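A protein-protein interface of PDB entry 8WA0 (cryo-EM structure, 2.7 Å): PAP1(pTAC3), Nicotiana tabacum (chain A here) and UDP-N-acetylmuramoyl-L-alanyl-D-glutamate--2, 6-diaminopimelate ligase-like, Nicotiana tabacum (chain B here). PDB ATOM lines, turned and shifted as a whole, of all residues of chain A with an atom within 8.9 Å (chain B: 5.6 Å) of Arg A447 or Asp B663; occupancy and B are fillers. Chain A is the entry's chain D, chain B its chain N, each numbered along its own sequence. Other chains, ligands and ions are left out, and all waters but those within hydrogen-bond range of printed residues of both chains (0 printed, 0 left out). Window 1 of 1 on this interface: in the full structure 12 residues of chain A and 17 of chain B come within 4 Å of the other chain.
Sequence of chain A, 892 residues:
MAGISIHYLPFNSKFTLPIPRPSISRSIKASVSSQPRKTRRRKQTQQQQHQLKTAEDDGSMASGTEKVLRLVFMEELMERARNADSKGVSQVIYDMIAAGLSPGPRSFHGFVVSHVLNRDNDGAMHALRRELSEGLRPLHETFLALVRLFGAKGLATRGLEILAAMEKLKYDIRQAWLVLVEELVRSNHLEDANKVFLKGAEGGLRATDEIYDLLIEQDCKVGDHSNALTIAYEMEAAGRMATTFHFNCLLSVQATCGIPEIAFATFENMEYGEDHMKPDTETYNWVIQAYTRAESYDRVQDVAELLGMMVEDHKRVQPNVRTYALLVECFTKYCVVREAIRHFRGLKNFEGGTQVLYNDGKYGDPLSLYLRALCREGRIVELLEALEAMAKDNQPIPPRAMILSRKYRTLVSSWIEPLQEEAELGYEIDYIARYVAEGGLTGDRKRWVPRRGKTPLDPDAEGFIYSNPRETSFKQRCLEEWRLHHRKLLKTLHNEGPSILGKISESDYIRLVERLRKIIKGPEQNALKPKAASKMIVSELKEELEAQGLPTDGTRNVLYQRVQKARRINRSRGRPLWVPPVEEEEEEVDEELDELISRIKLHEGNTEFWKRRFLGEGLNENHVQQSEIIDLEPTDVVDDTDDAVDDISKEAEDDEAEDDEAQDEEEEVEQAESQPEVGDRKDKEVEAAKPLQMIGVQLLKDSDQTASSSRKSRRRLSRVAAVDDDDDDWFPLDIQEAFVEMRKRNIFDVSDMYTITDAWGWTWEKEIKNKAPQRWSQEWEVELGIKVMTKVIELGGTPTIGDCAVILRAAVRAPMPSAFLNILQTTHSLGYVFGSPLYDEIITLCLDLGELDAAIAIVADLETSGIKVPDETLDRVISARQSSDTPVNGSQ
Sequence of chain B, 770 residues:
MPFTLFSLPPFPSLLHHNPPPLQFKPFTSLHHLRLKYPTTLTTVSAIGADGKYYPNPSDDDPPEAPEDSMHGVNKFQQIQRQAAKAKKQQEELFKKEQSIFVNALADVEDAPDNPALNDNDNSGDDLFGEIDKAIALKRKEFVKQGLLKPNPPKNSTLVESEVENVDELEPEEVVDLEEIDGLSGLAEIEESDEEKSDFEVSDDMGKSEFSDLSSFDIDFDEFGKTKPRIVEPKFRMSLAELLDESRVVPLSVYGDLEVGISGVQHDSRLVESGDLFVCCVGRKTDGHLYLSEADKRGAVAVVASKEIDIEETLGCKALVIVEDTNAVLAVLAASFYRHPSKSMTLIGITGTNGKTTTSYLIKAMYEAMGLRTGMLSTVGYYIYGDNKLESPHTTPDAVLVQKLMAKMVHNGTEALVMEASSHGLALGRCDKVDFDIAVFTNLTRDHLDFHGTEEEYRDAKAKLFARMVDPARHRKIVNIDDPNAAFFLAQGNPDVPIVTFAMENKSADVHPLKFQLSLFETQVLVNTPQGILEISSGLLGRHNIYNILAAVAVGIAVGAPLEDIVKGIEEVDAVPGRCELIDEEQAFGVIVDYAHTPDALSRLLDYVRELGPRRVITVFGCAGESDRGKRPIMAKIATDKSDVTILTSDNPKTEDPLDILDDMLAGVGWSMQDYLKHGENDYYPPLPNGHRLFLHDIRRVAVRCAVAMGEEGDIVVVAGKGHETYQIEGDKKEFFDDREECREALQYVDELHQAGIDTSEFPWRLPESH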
ATOM      1  N   TYR A 431       2.265 -22.947   6.512  1.00  0.00           N
ATOM      2  CA  TYR A 431       2.899 -23.261   5.277  1.00  0.00           C
ATOM      3  C   TYR A 431       3.870 -24.422   5.387  1.00  0.00           C
ATOM      4  O   TYR A 431       3.877 -25.312   4.533  1.00  0.00           O
ATOM      5  CB  TYR A 431       3.584 -22.003   4.773  1.00  0.00           C
ATOM      6  CG  TYR A 431       2.607 -20.949   4.327  1.00  0.00           C
ATOM      7  CD1 TYR A 431       1.898 -21.096   3.147  1.00  0.00           C
ATOM      8  CD2 TYR A 431       2.389 -19.811   5.087  1.00  0.00           C
ATOM      9  CE1 TYR A 431       0.997 -20.137   2.731  1.00  0.00           C
ATOM     10  CE2 TYR A 431       1.489 -18.845   4.680  1.00  0.00           C
ATOM     11  CZ  TYR A 431       0.797 -19.014   3.500  1.00  0.00           C
ATOM     12  OH  TYR A 431      -0.101 -18.056   3.089  1.00  0.00           O
ATOM     13  N   ILE A 432       4.677 -24.436   6.438  1.00  0.00           N
ATOM     14  CA  ILE A 432       5.649 -25.508   6.616  1.00  0.00           C
ATOM     15  C   ILE A 432       4.944 -26.829   6.824  1.00  0.00           C
ATOM     16  O   ILE A 432       5.404 -27.872   6.373  1.00  0.00           O
ATOM     17  CB  ILE A 432       6.648 -25.224   7.738  1.00  0.00           C
ATOM     18  CG1 ILE A 432       5.952 -24.520   8.903  1.00  0.00           C
ATOM     19  CG2 ILE A 432       7.781 -24.354   7.221  1.00  0.00           C
ATOM     20  CD1 ILE A 432       6.890 -24.114  10.017  1.00  0.00           C
ATOM     21  N   TYR A 435       4.000 -28.421   3.613  1.00  0.00           N
ATOM     22  CA  TYR A 435       5.096 -29.041   2.907  1.00  0.00           C
ATOM     23  C   TYR A 435       5.416 -30.366   3.498  1.00  0.00           C
ATOM     24  O   TYR A 435       5.590 -31.338   2.783  1.00  0.00           O
ATOM     25  CB  TYR A 435       6.378 -28.220   2.906  1.00  0.00           C
ATOM     26  CG  TYR A 435       7.503 -28.978   2.240  1.00  0.00           C
ATOM     27  CD1 TYR A 435       7.545 -29.120   0.865  1.00  0.00           C
ATOM     28  CD2 TYR A 435       8.486 -29.607   2.988  1.00  0.00           C
ATOM     29  CE1 TYR A 435       8.549 -29.839   0.256  1.00  0.00           C
ATOM     30  CE2 TYR A 435       9.514 -30.304   2.386  1.00  0.00           C
ATOM     31  CZ  TYR A 435       9.541 -30.417   1.017  1.00  0.00           C
ATOM     32  OH  TYR A 435      10.550 -31.130   0.409  1.00  0.00           O
ATOM     33  N   VAL A 436       5.447 -30.441   4.808  1.00  0.00           N
ATOM     34  CA  VAL A 436       5.862 -31.688   5.374  1.00  0.00           C
ATOM     35  C   VAL A 436       4.883 -32.758   4.962  1.00  0.00           C
ATOM     36  O   VAL A 436       5.266 -33.896   4.735  1.00  0.00           O
ATOM     37  CB  VAL A 436       6.123 -31.634   6.894  1.00  0.00           C
ATOM     38  CG1 VAL A 436       7.166 -30.578   7.218  1.00  0.00           C
ATOM     39  CG2 VAL A 436       4.856 -31.427   7.702  1.00  0.00           C
ATOM     40  N   GLU A 438       2.997 -33.179   2.168  1.00  0.00           N
ATOM     41  CA  GLU A 438       3.102 -33.708   0.810  1.00  0.00           C
ATOM     42  C   GLU A 438       4.381 -34.478   0.572  1.00  0.00           C
ATOM     43  O   GLU A 438       4.342 -35.601   0.076  1.00  0.00           O
ATOM     44  CB  GLU A 438       2.988 -32.572  -0.202  1.00  0.00           C
ATOM     45  CG  GLU A 438       1.822 -31.634   0.059  1.00  0.00           C
ATOM     46  CD  GLU A 438       0.484 -32.346   0.050  1.00  0.00           C
ATOM     47  OE1 GLU A 438       0.181 -33.036  -0.946  1.00  0.00           O
ATOM     48  OE2 GLU A 438      -0.267 -32.209   1.037  1.00  0.00           O
ATOM     49  N   GLY A 439       5.517 -33.895   0.930  1.00  0.00           N
ATOM     50  CA  GLY A 439       6.783 -34.601   0.840  1.00  0.00           C
ATOM     51  C   GLY A 439       7.704 -33.845   1.756  1.00  0.00           C
ATOM     52  O   GLY A 439       7.749 -32.645   1.671  1.00  0.00           O
ATOM     53  N   GLY A 440       8.421 -34.510   2.636  1.00  0.00           N
ATOM     54  CA  GLY A 440       9.397 -33.822   3.459  1.00  0.00           C
ATOM     55  C   GLY A 440      10.447 -34.846   3.800  1.00  0.00           C
ATOM     56  O   GLY A 440      10.072 -35.985   4.074  1.00  0.00           O
ATOM     57  N   LEU A 441      11.726 -34.470   3.791  1.00  0.00           N
ATOM     58  CA  LEU A 441      12.836 -35.401   4.067  1.00  0.00           C
ATOM     59  C   LEU A 441      13.014 -36.412   2.942  1.00  0.00           C
ATOM     60  O   LEU A 441      14.095 -36.511   2.368  1.00  0.00           O
ATOM     61  CB  LEU A 441      12.721 -36.081   5.442  1.00  0.00           C
ATOM     62  CG  LEU A 441      13.744 -37.169   5.782  1.00  0.00           C
ATOM     63  CD1 LEU A 441      15.163 -36.619   5.798  1.00  0.00           C
ATOM     64  CD2 LEU A 441      13.407 -37.815   7.115  1.00  0.00           C
ATOM     65  N   THR A 442      11.979 -37.183   2.645  1.00  0.00           N
ATOM     66  CA  THR A 442      12.023 -38.129   1.550  1.00  0.00           C
ATOM     67  C   THR A 442      10.635 -38.079   0.958  1.00  0.00           C
ATOM     68  O   THR A 442       9.699 -37.651   1.627  1.00  0.00           O
ATOM     69  CB  THR A 442      12.301 -39.560   2.039  1.00  0.00           C
ATOM     70  OG1 THR A 442      11.725 -39.741   3.338  1.00  0.00           O
ATOM     71  CG2 THR A 442      13.798 -39.831   2.114  1.00  0.00           C
ATOM     72  N   GLY A 443      10.474 -38.506  -0.286  1.00  0.00           N
ATOM     73  CA  GLY A 443       9.145 -38.558  -0.873  1.00  0.00           C
ATOM     74  C   GLY A 443       8.942 -37.716  -2.110  1.00  0.00           C
ATOM     75  O   GLY A 443       9.813 -36.942  -2.494  1.00  0.00           O
ATOM     76  N   ASP A 444       7.780 -37.843  -2.737  1.00  0.00           N
ATOM     77  CA  ASP A 444       7.558 -37.135  -3.991  1.00  0.00           C
ATOM     78  C   ASP A 444       6.514 -36.046  -3.907  1.00  0.00           C
ATOM     79  O   ASP A 444       5.411 -36.268  -3.412  1.00  0.00           O
ATOM     80  CB  ASP A 444       7.181 -38.126  -5.096  1.00  0.00           C
ATOM     81  CG  ASP A 444       7.231 -37.508  -6.482  1.00  0.00           C
ATOM     82  OD1 ASP A 444       8.014 -36.556  -6.688  1.00  0.00           O
ATOM     83  OD2 ASP A 444       6.497 -37.984  -7.372  1.00  0.00           O
ATOM     84  N   ARG A 445       6.857 -34.865  -4.395  1.00  0.00           N
ATOM     85  CA  ARG A 445       5.910 -33.771  -4.424  1.00  0.00           C
ATOM     86  C   ARG A 445       5.991 -33.293  -5.852  1.00  0.00           C
ATOM     87  O   ARG A 445       7.044 -33.387  -6.473  1.00  0.00           O
ATOM     88  CB  ARG A 445       6.347 -32.664  -3.466  1.00  0.00           C
ATOM     89  N   LYS A 446       4.896 -32.785  -6.386  1.00  0.00           N
ATOM     90  CA  LYS A 446       4.903 -32.369  -7.756  1.00  0.00           C
ATOM     91  C   LYS A 446       5.466 -31.008  -7.693  1.00  0.00           C
ATOM     92  O   LYS A 446       4.727 -30.036  -7.659  1.00  0.00           O
ATOM     93  CB  LYS A 446       3.476 -32.299  -8.285  1.00  0.00           C
ATOM     94  N   ARG A 447       6.783 -30.908  -7.673  1.00  0.00           N
ATOM     95  CA  ARG A 447       7.343 -29.603  -7.502  1.00  0.00           C
ATOM     96  C   ARG A 447       6.899 -28.804  -8.707  1.00  0.00           C
ATOM     97  O   ARG A 447       7.116 -29.229  -9.835  1.00  0.00           O
ATOM     98  CB  ARG A 447       8.845 -29.739  -7.390  1.00  0.00           C
ATOM     99  CG  ARG A 447       9.280 -30.861  -6.478  1.00  0.00           C
ATOM    100  CD  ARG A 447      10.794 -30.948  -6.389  1.00  0.00           C
ATOM    101  NE  ARG A 447      11.225 -32.105  -5.609  1.00  0.00           N
ATOM    102  CZ  ARG A 447      11.529 -32.069  -4.316  1.00  0.00           C
ATOM    103  NH1 ARG A 447      11.464 -30.926  -3.647  1.00  0.00           N
ATOM    104  NH2 ARG A 447      11.910 -33.175  -3.692  1.00  0.00           N
ATOM    105  N   TRP A 448       6.293 -27.645  -8.499  1.00  0.00           N
ATOM    106  CA  TRP A 448       5.765 -26.894  -9.626  1.00  0.00           C
ATOM    107  C   TRP A 448       6.756 -25.977 -10.295  1.00  0.00           C
ATOM    108  O   TRP A 448       6.591 -24.770 -10.233  1.00  0.00           O
ATOM    109  CB  TRP A 448       4.532 -26.073  -9.254  1.00  0.00           C
ATOM    110  CG  TRP A 448       3.393 -26.842  -8.691  1.00  0.00           C
ATOM    111  CD1 TRP A 448       3.342 -27.459  -7.481  1.00  0.00           C
ATOM    112  CD2 TRP A 448       2.107 -27.026  -9.288  1.00  0.00           C
ATOM    113  NE1 TRP A 448       2.118 -28.051  -7.299  1.00  0.00           N
ATOM    114  CE2 TRP A 448       1.338 -27.795  -8.394  1.00  0.00           C
ATOM    115  CE3 TRP A 448       1.535 -26.632 -10.499  1.00  0.00           C
ATOM    116  CZ2 TRP A 448       0.028 -28.173  -8.672  1.00  0.00           C
ATOM    117  CZ3 TRP A 448       0.236 -27.009 -10.774  1.00  0.00           C
ATOM    118  CH2 TRP A 448      -0.504 -27.770  -9.864  1.00  0.00           C
ATOM    119  N   VAL A 449       7.782 -26.529 -10.936  1.00  0.00           N
ATOM    120  CA  VAL A 449       8.745 -25.722 -11.694  1.00  0.00           C
ATOM    121  C   VAL A 449       8.533 -25.965 -13.186  1.00  0.00           C
ATOM    122  O   VAL A 449       8.429 -27.113 -13.623  1.00  0.00           O
ATOM    123  CB  VAL A 449      10.164 -26.102 -11.334  1.00  0.00           C
ATOM    124  N   PRO A 450       8.414 -24.893 -13.976  1.00  0.00           N
ATOM    125  CA  PRO A 450       8.139 -25.084 -15.399  1.00  0.00           C
ATOM    126  C   PRO A 450       9.264 -25.753 -16.162  1.00  0.00           C
ATOM    127  O   PRO A 450      10.431 -25.448 -15.916  1.00  0.00           O
ATOM    128  CB  PRO A 450       7.945 -23.663 -15.899  1.00  0.00           C
ATOM    129  CG  PRO A 450       7.401 -22.955 -14.716  1.00  0.00           C
ATOM    130  CD  PRO A 450       8.200 -23.499 -13.568  1.00  0.00           C
ATOM    131  N   ARG A 451       8.922 -26.637 -17.095  1.00  0.00           N
ATOM    132  CA  ARG A 451       9.928 -27.360 -17.870  1.00  0.00           C
ATOM    133  C   ARG A 451       9.613 -27.300 -19.356  1.00  0.00           C
ATOM    134  O   ARG A 451       8.462 -27.101 -19.739  1.00  0.00           O
ATOM    135  CB  ARG A 451      10.014 -28.825 -17.423  1.00  0.00           C
ATOM    136  CG  ARG A 451      10.416 -29.043 -15.971  1.00  0.00           C
ATOM    137  CD  ARG A 451      11.822 -28.538 -15.682  1.00  0.00           C
ATOM    138  NE  ARG A 451      12.201 -28.753 -14.287  1.00  0.00           N
ATOM    139  CZ  ARG A 451      13.350 -28.353 -13.751  1.00  0.00           C
ATOM    140  NH1 ARG A 451      14.242 -27.709 -14.490  1.00  0.00           N
ATOM    141  NH2 ARG A 451      13.607 -28.595 -12.472  1.00  0.00           N
ATOM    142  N   LEU A 457       1.660 -29.161 -16.894  1.00  0.00           N
ATOM    143  CA  LEU A 457       2.048 -29.029 -15.478  1.00  0.00           C
ATOM    144  C   LEU A 457       0.965 -29.337 -14.490  1.00  0.00           C
ATOM    145  O   LEU A 457       1.231 -29.972 -13.482  1.00  0.00           O
ATOM    146  CB  LEU A 457       2.667 -27.671 -15.164  1.00  0.00           C
ATOM    147  N   ASP A 458      -0.257 -28.902 -14.758  1.00  0.00           N
ATOM    148  CA  ASP A 458      -1.354 -29.262 -13.880  1.00  0.00           C
ATOM    149  C   ASP A 458      -1.498 -30.739 -13.981  1.00  0.00           C
ATOM    150  O   ASP A 458      -1.535 -31.288 -15.084  1.00  0.00           O
ATOM    151  CB  ASP A 458      -2.643 -28.646 -14.366  1.00  0.00           C
ATOM    152  CG  ASP A 458      -3.525 -28.166 -13.233  1.00  0.00           C
ATOM    153  OD1 ASP A 458      -3.227 -28.483 -12.065  1.00  0.00           O
ATOM    154  OD2 ASP A 458      -4.523 -27.470 -13.514  1.00  0.00           O
ATOM    155  N   PRO A 459      -1.599 -31.416 -12.845  1.00  0.00           N
ATOM    156  CA  PRO A 459      -1.863 -32.837 -12.924  1.00  0.00           C
ATOM    157  C   PRO A 459      -3.272 -32.952 -13.378  1.00  0.00           C
ATOM    158  O   PRO A 459      -3.696 -34.006 -13.818  1.00  0.00           O
ATOM    159  CB  PRO A 459      -1.728 -33.306 -11.485  1.00  0.00           C
ATOM    160  CG  PRO A 459      -1.772 -32.080 -10.637  1.00  0.00           C
ATOM    161  CD  PRO A 459      -1.205 -30.997 -11.492  1.00  0.00           C
ATOM    162  N   ARG B 628      15.480 -32.840   2.845  1.00  0.00           N
ATOM    163  CA  ARG B 628      14.434 -32.178   2.074  1.00  0.00           C
ATOM    164  C   ARG B 628      13.549 -31.308   2.956  1.00  0.00           C
ATOM    165  O   ARG B 628      13.068 -30.260   2.507  1.00  0.00           O
ATOM    166  CB  ARG B 628      13.593 -33.214   1.331  1.00  0.00           C
ATOM    167  CG  ARG B 628      14.385 -34.052   0.338  1.00  0.00           C
ATOM    168  CD  ARG B 628      13.490 -35.032  -0.398  1.00  0.00           C
ATOM    169  NE  ARG B 628      14.233 -35.828  -1.370  1.00  0.00           N
ATOM    170  CZ  ARG B 628      13.687 -36.756  -2.150  1.00  0.00           C
ATOM    171  NH1 ARG B 628      14.441 -37.432  -3.006  1.00  0.00           N
ATOM    172  NH2 ARG B 628      12.388 -37.008  -2.072  1.00  0.00           N
ATOM    173  N   GLY B 629      13.323 -31.716   4.205  1.00  0.00           N
ATOM    174  CA  GLY B 629      12.546 -30.908   5.126  1.00  0.00           C
ATOM    175  C   GLY B 629      13.261 -29.678   5.640  1.00  0.00           C
ATOM    176  O   GLY B 629      12.621 -28.829   6.273  1.00  0.00           O
ATOM    177  N   ARG B 631      14.819 -27.363   3.692  1.00  0.00           N
ATOM    178  CA  ARG B 631      14.607 -26.225   2.799  1.00  0.00           C
ATOM    179  C   ARG B 631      13.376 -25.398   3.156  1.00  0.00           C
ATOM    180  O   ARG B 631      13.494 -24.162   3.232  1.00  0.00           O
ATOM    181  CB  ARG B 631      14.546 -26.718   1.350  1.00  0.00           C
ATOM    182  N   PRO B 632      12.186 -25.978   3.377  1.00  0.00           N
ATOM    183  CA  PRO B 632      11.024 -25.117   3.652  1.00  0.00           C
ATOM    184  C   PRO B 632      11.128 -24.369   4.968  1.00  0.00           C
ATOM    185  O   PRO B 632      10.760 -23.189   5.029  1.00  0.00           O
ATOM    186  CB  PRO B 632       9.849 -26.105   3.645  1.00  0.00           C
ATOM    187  CG  PRO B 632      10.457 -27.406   4.006  1.00  0.00           C
ATOM    188  CD  PRO B 632      11.807 -27.402   3.356  1.00  0.00           C
ATOM    189  N   ASP B 659      14.690 -27.161  -9.102  1.00  0.00           N
ATOM    190  CA  ASP B 659      13.894 -28.147  -8.384  1.00  0.00           C
ATOM    191  C   ASP B 659      13.911 -27.906  -6.881  1.00  0.00           C
ATOM    192  O   ASP B 659      12.852 -27.768  -6.262  1.00  0.00           O
ATOM    193  CB  ASP B 659      14.399 -29.561  -8.693  1.00  0.00           C
ATOM    194  N   ILE B 660      15.102 -27.851  -6.280  1.00  0.00           N
ATOM    195  CA  ILE B 660      15.203 -27.472  -4.876  1.00  0.00           C
ATOM    196  C   ILE B 660      14.817 -26.010  -4.697  1.00  0.00           C
ATOM    197  O   ILE B 660      14.308 -25.618  -3.638  1.00  0.00           O
ATOM    198  CB  ILE B 660      16.620 -27.768  -4.349  1.00  0.00           C
ATOM    199  CG1 ILE B 660      16.717 -27.469  -2.851  1.00  0.00           C
ATOM    200  CG2 ILE B 660      17.665 -26.986  -5.134  1.00  0.00           C
ATOM    201  CD1 ILE B 660      15.774 -28.292  -2.001  1.00  0.00           C
ATOM    202  N   LEU B 661      15.039 -25.184  -5.722  1.00  0.00           N
ATOM    203  CA  LEU B 661      14.574 -23.802  -5.672  1.00  0.00           C
ATOM    204  C   LEU B 661      13.055 -23.743  -5.558  1.00  0.00           C
ATOM    205  O   LEU B 661      12.512 -22.939  -4.792  1.00  0.00           O
ATOM    206  CB  LEU B 661      15.051 -23.043  -6.910  1.00  0.00           C
ATOM    207  CG  LEU B 661      15.827 -21.751  -6.655  1.00  0.00           C
ATOM    208  CD1 LEU B 661      16.229 -21.096  -7.967  1.00  0.00           C
ATOM    209  CD2 LEU B 661      15.007 -20.796  -5.805  1.00  0.00           C
ATOM    210  N   ASP B 662      12.352 -24.595  -6.309  1.00  0.00           N
ATOM    211  CA  ASP B 662      10.905 -24.684  -6.154  1.00  0.00           C
ATOM    212  C   ASP B 662      10.526 -25.198  -4.773  1.00  0.00           C
ATOM    213  O   ASP B 662       9.495 -24.794  -4.223  1.00  0.00           O
ATOM    214  CB  ASP B 662      10.313 -25.583  -7.241  1.00  0.00           C
ATOM    215  CG  ASP B 662       8.797 -25.609  -7.213  1.00  0.00           C
ATOM    216  OD1 ASP B 662       8.178 -24.579  -7.554  1.00  0.00           O
ATOM    217  OD2 ASP B 662       8.227 -26.658  -6.849  1.00  0.00           O
ATOM    218  N   ASP B 663      11.348 -26.076  -4.193  1.00  0.00           N
ATOM    219  CA  ASP B 663      11.094 -26.541  -2.834  1.00  0.00           C
ATOM    220  C   ASP B 663      11.175 -25.390  -1.838  1.00  0.00           C
ATOM    221  O   ASP B 663      10.335 -25.277  -0.938  1.00  0.00           O
ATOM    222  CB  ASP B 663      12.085 -27.646  -2.467  1.00  0.00           C
ATOM    223  CG  ASP B 663      11.746 -28.327  -1.154  1.00  0.00           C
ATOM    224  OD1 ASP B 663      10.660 -28.061  -0.601  1.00  0.00           O
ATOM    225  OD2 ASP B 663      12.572 -29.132  -0.674  1.00  0.00           O
ATOM    226  N   MET B 664      12.178 -24.522  -1.987  1.00  0.00           N
ATOM    227  CA  MET B 664      12.273 -23.354  -1.115  1.00  0.00           C
ATOM    228  C   MET B 664      11.125 -22.384  -1.363  1.00  0.00           C
ATOM    229  O   MET B 664      10.613 -21.765  -0.422  1.00  0.00           O
ATOM    230  CB  MET B 664      13.616 -22.649  -1.308  1.00  0.00           C
ATOM    231  CG  MET B 664      14.723 -23.138  -0.381  1.00  0.00           C
ATOM    232  SD  MET B 664      15.761 -24.416  -1.114  1.00  0.00           S
ATOM    233  CE  MET B 664      16.535 -23.502  -2.446  1.00  0.00           C
ATOM    234  N   LEU B 665      10.710 -22.233  -2.624  1.00  0.00           N
ATOM    235  CA  LEU B 665       9.601 -21.335  -2.933  1.00  0.00           C
ATOM    236  C   LEU B 665       8.285 -21.845  -2.360  1.00  0.00           C
ATOM    237  O   LEU B 665       7.417 -21.042  -1.999  1.00  0.00           O
ATOM    238  CB  LEU B 665       9.482 -21.147  -4.444  1.00  0.00           C
ATOM    239  CG  LEU B 665      10.081 -19.863  -5.020  1.00  0.00           C
ATOM    240  CD1 LEU B 665       9.371 -18.642  -4.453  1.00  0.00           C
ATOM    241  CD2 LEU B 665      11.573 -19.790  -4.748  1.00  0.00           C
ATOM    242  N   ALA B 666       8.119 -23.166  -2.270  1.00  0.00           N
ATOM    243  CA  ALA B 666       6.895 -23.727  -1.712  1.00  0.00           C
ATOM    244  C   ALA B 666       6.732 -23.413  -0.231  1.00  0.00           C
ATOM    245  O   ALA B 666       5.630 -23.576   0.306  1.00  0.00           O
ATOM    246  CB  ALA B 666       6.864 -25.241  -1.926  1.00  0.00           C
ATOM    247  N   GLY B 667       7.796 -22.970   0.440  1.00  0.00           N
ATOM    248  CA  GLY B 667       7.683 -22.642   1.851  1.00  0.00           C
ATOM    249  C   GLY B 667       6.803 -21.433   2.106  1.00  0.00           C
ATOM    250  O   GLY B 667       6.075 -21.385   3.102  1.00  0.00           O
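The side-chain hydroxyl of Tyr A435 sits close to the backbone carbonyl oxygen of Gly A439 (3.4 Å).
NE1 of Trp A448 sits close to O of Lys A446, at 3.3 Å.
Glu A438 touches none of the printed residues of chain B.
Of the printed residues of chain B, Gly A443 touches Arg B628 (2.6 Å).
Arg A447 touches just these residues of chain B: Asp B659, Asp B662 and Asp B663.
Printed residues of chain A within 4 Å of Arg B628: Tyr A435, Leu A441, Thr A442 and Gly A443.
Asp B662 touches three residues of chain A.
Asp B663 touches just these residues of chain A: Tyr A435 (2.9 Å) and Arg A447 (3.5 Å).
Of the printed residues of chain A, Gly B667 touches Tyr A431 (3.1 Å).
The nearest printed residue of chain A that does not touch Asp B659 is Val A449 (5.2 Å).
The backbone NH (N) of Trp A448 lies within hydrogen-bond range of the side-chain carboxylate (OD2) of Asp B662.
The side-chain hydroxyl of Tyr A435 is in hydrogen-bond range of the backbone carbonyl oxygen of Arg B628 (3.4 Å).
The side-chain carboxylate (OD2) of Asp B663 is in hydrogen-bond range of the side-chain hydroxyl (OH) of Tyr A435, 3.0 Å away.
N of Leu A441 lies close to N of Gly B629, 3.2 Å away.
The guanidinium group (NH2) of Arg B628 is in hydrogen-bond range of the backbone carbonyl oxygen (O) of Gly A443 (2.6 Å).
OD2 of Asp B663 is in salt-bridge range of NH1 of Arg A447, 3.6 Å away.
Tyr A431 touches Gly B667 (CB to O, 3.1 Å).
Ile A432 touches Pro B632 (CG2 to O, 3.9 Å).
Tyr A435 touches Pro B632 (CD2 to CG, 3.1 Å).
Leu A441 touches Arg B628 (O to CD, 3.2 Å).
Thr A442 touches Arg B628 (C to NH2, 3.7 Å).
Arg A447 touches Asp B659.
Arg A447 touches Asp B662.
OD1 of Asp B662 touches N of Val A449, 3.9 Å away.
Arg A451 touches Asp B659 (NH2 to N, 3.8 Å).
Printed residues of chain B that touch a printed residue of chain A: Arg B628, Gly B629, Pro B632, Asp B659, Asp B662, Asp B663 and Gly B667.
Hydrophobic or aromatic side chains of chain A within 4 Å of the printed part of chain B: Tyr A431, Ile A432 and Tyr A435.
Among the printed residues, 15 pairs touch across the chains.
Among the printed residues, Asp or Glu carboxylates within 4 Å of a Lys or Arg side-chain nitrogen of the other chain: Arg A447 with Asp B663 (3.6 Å).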
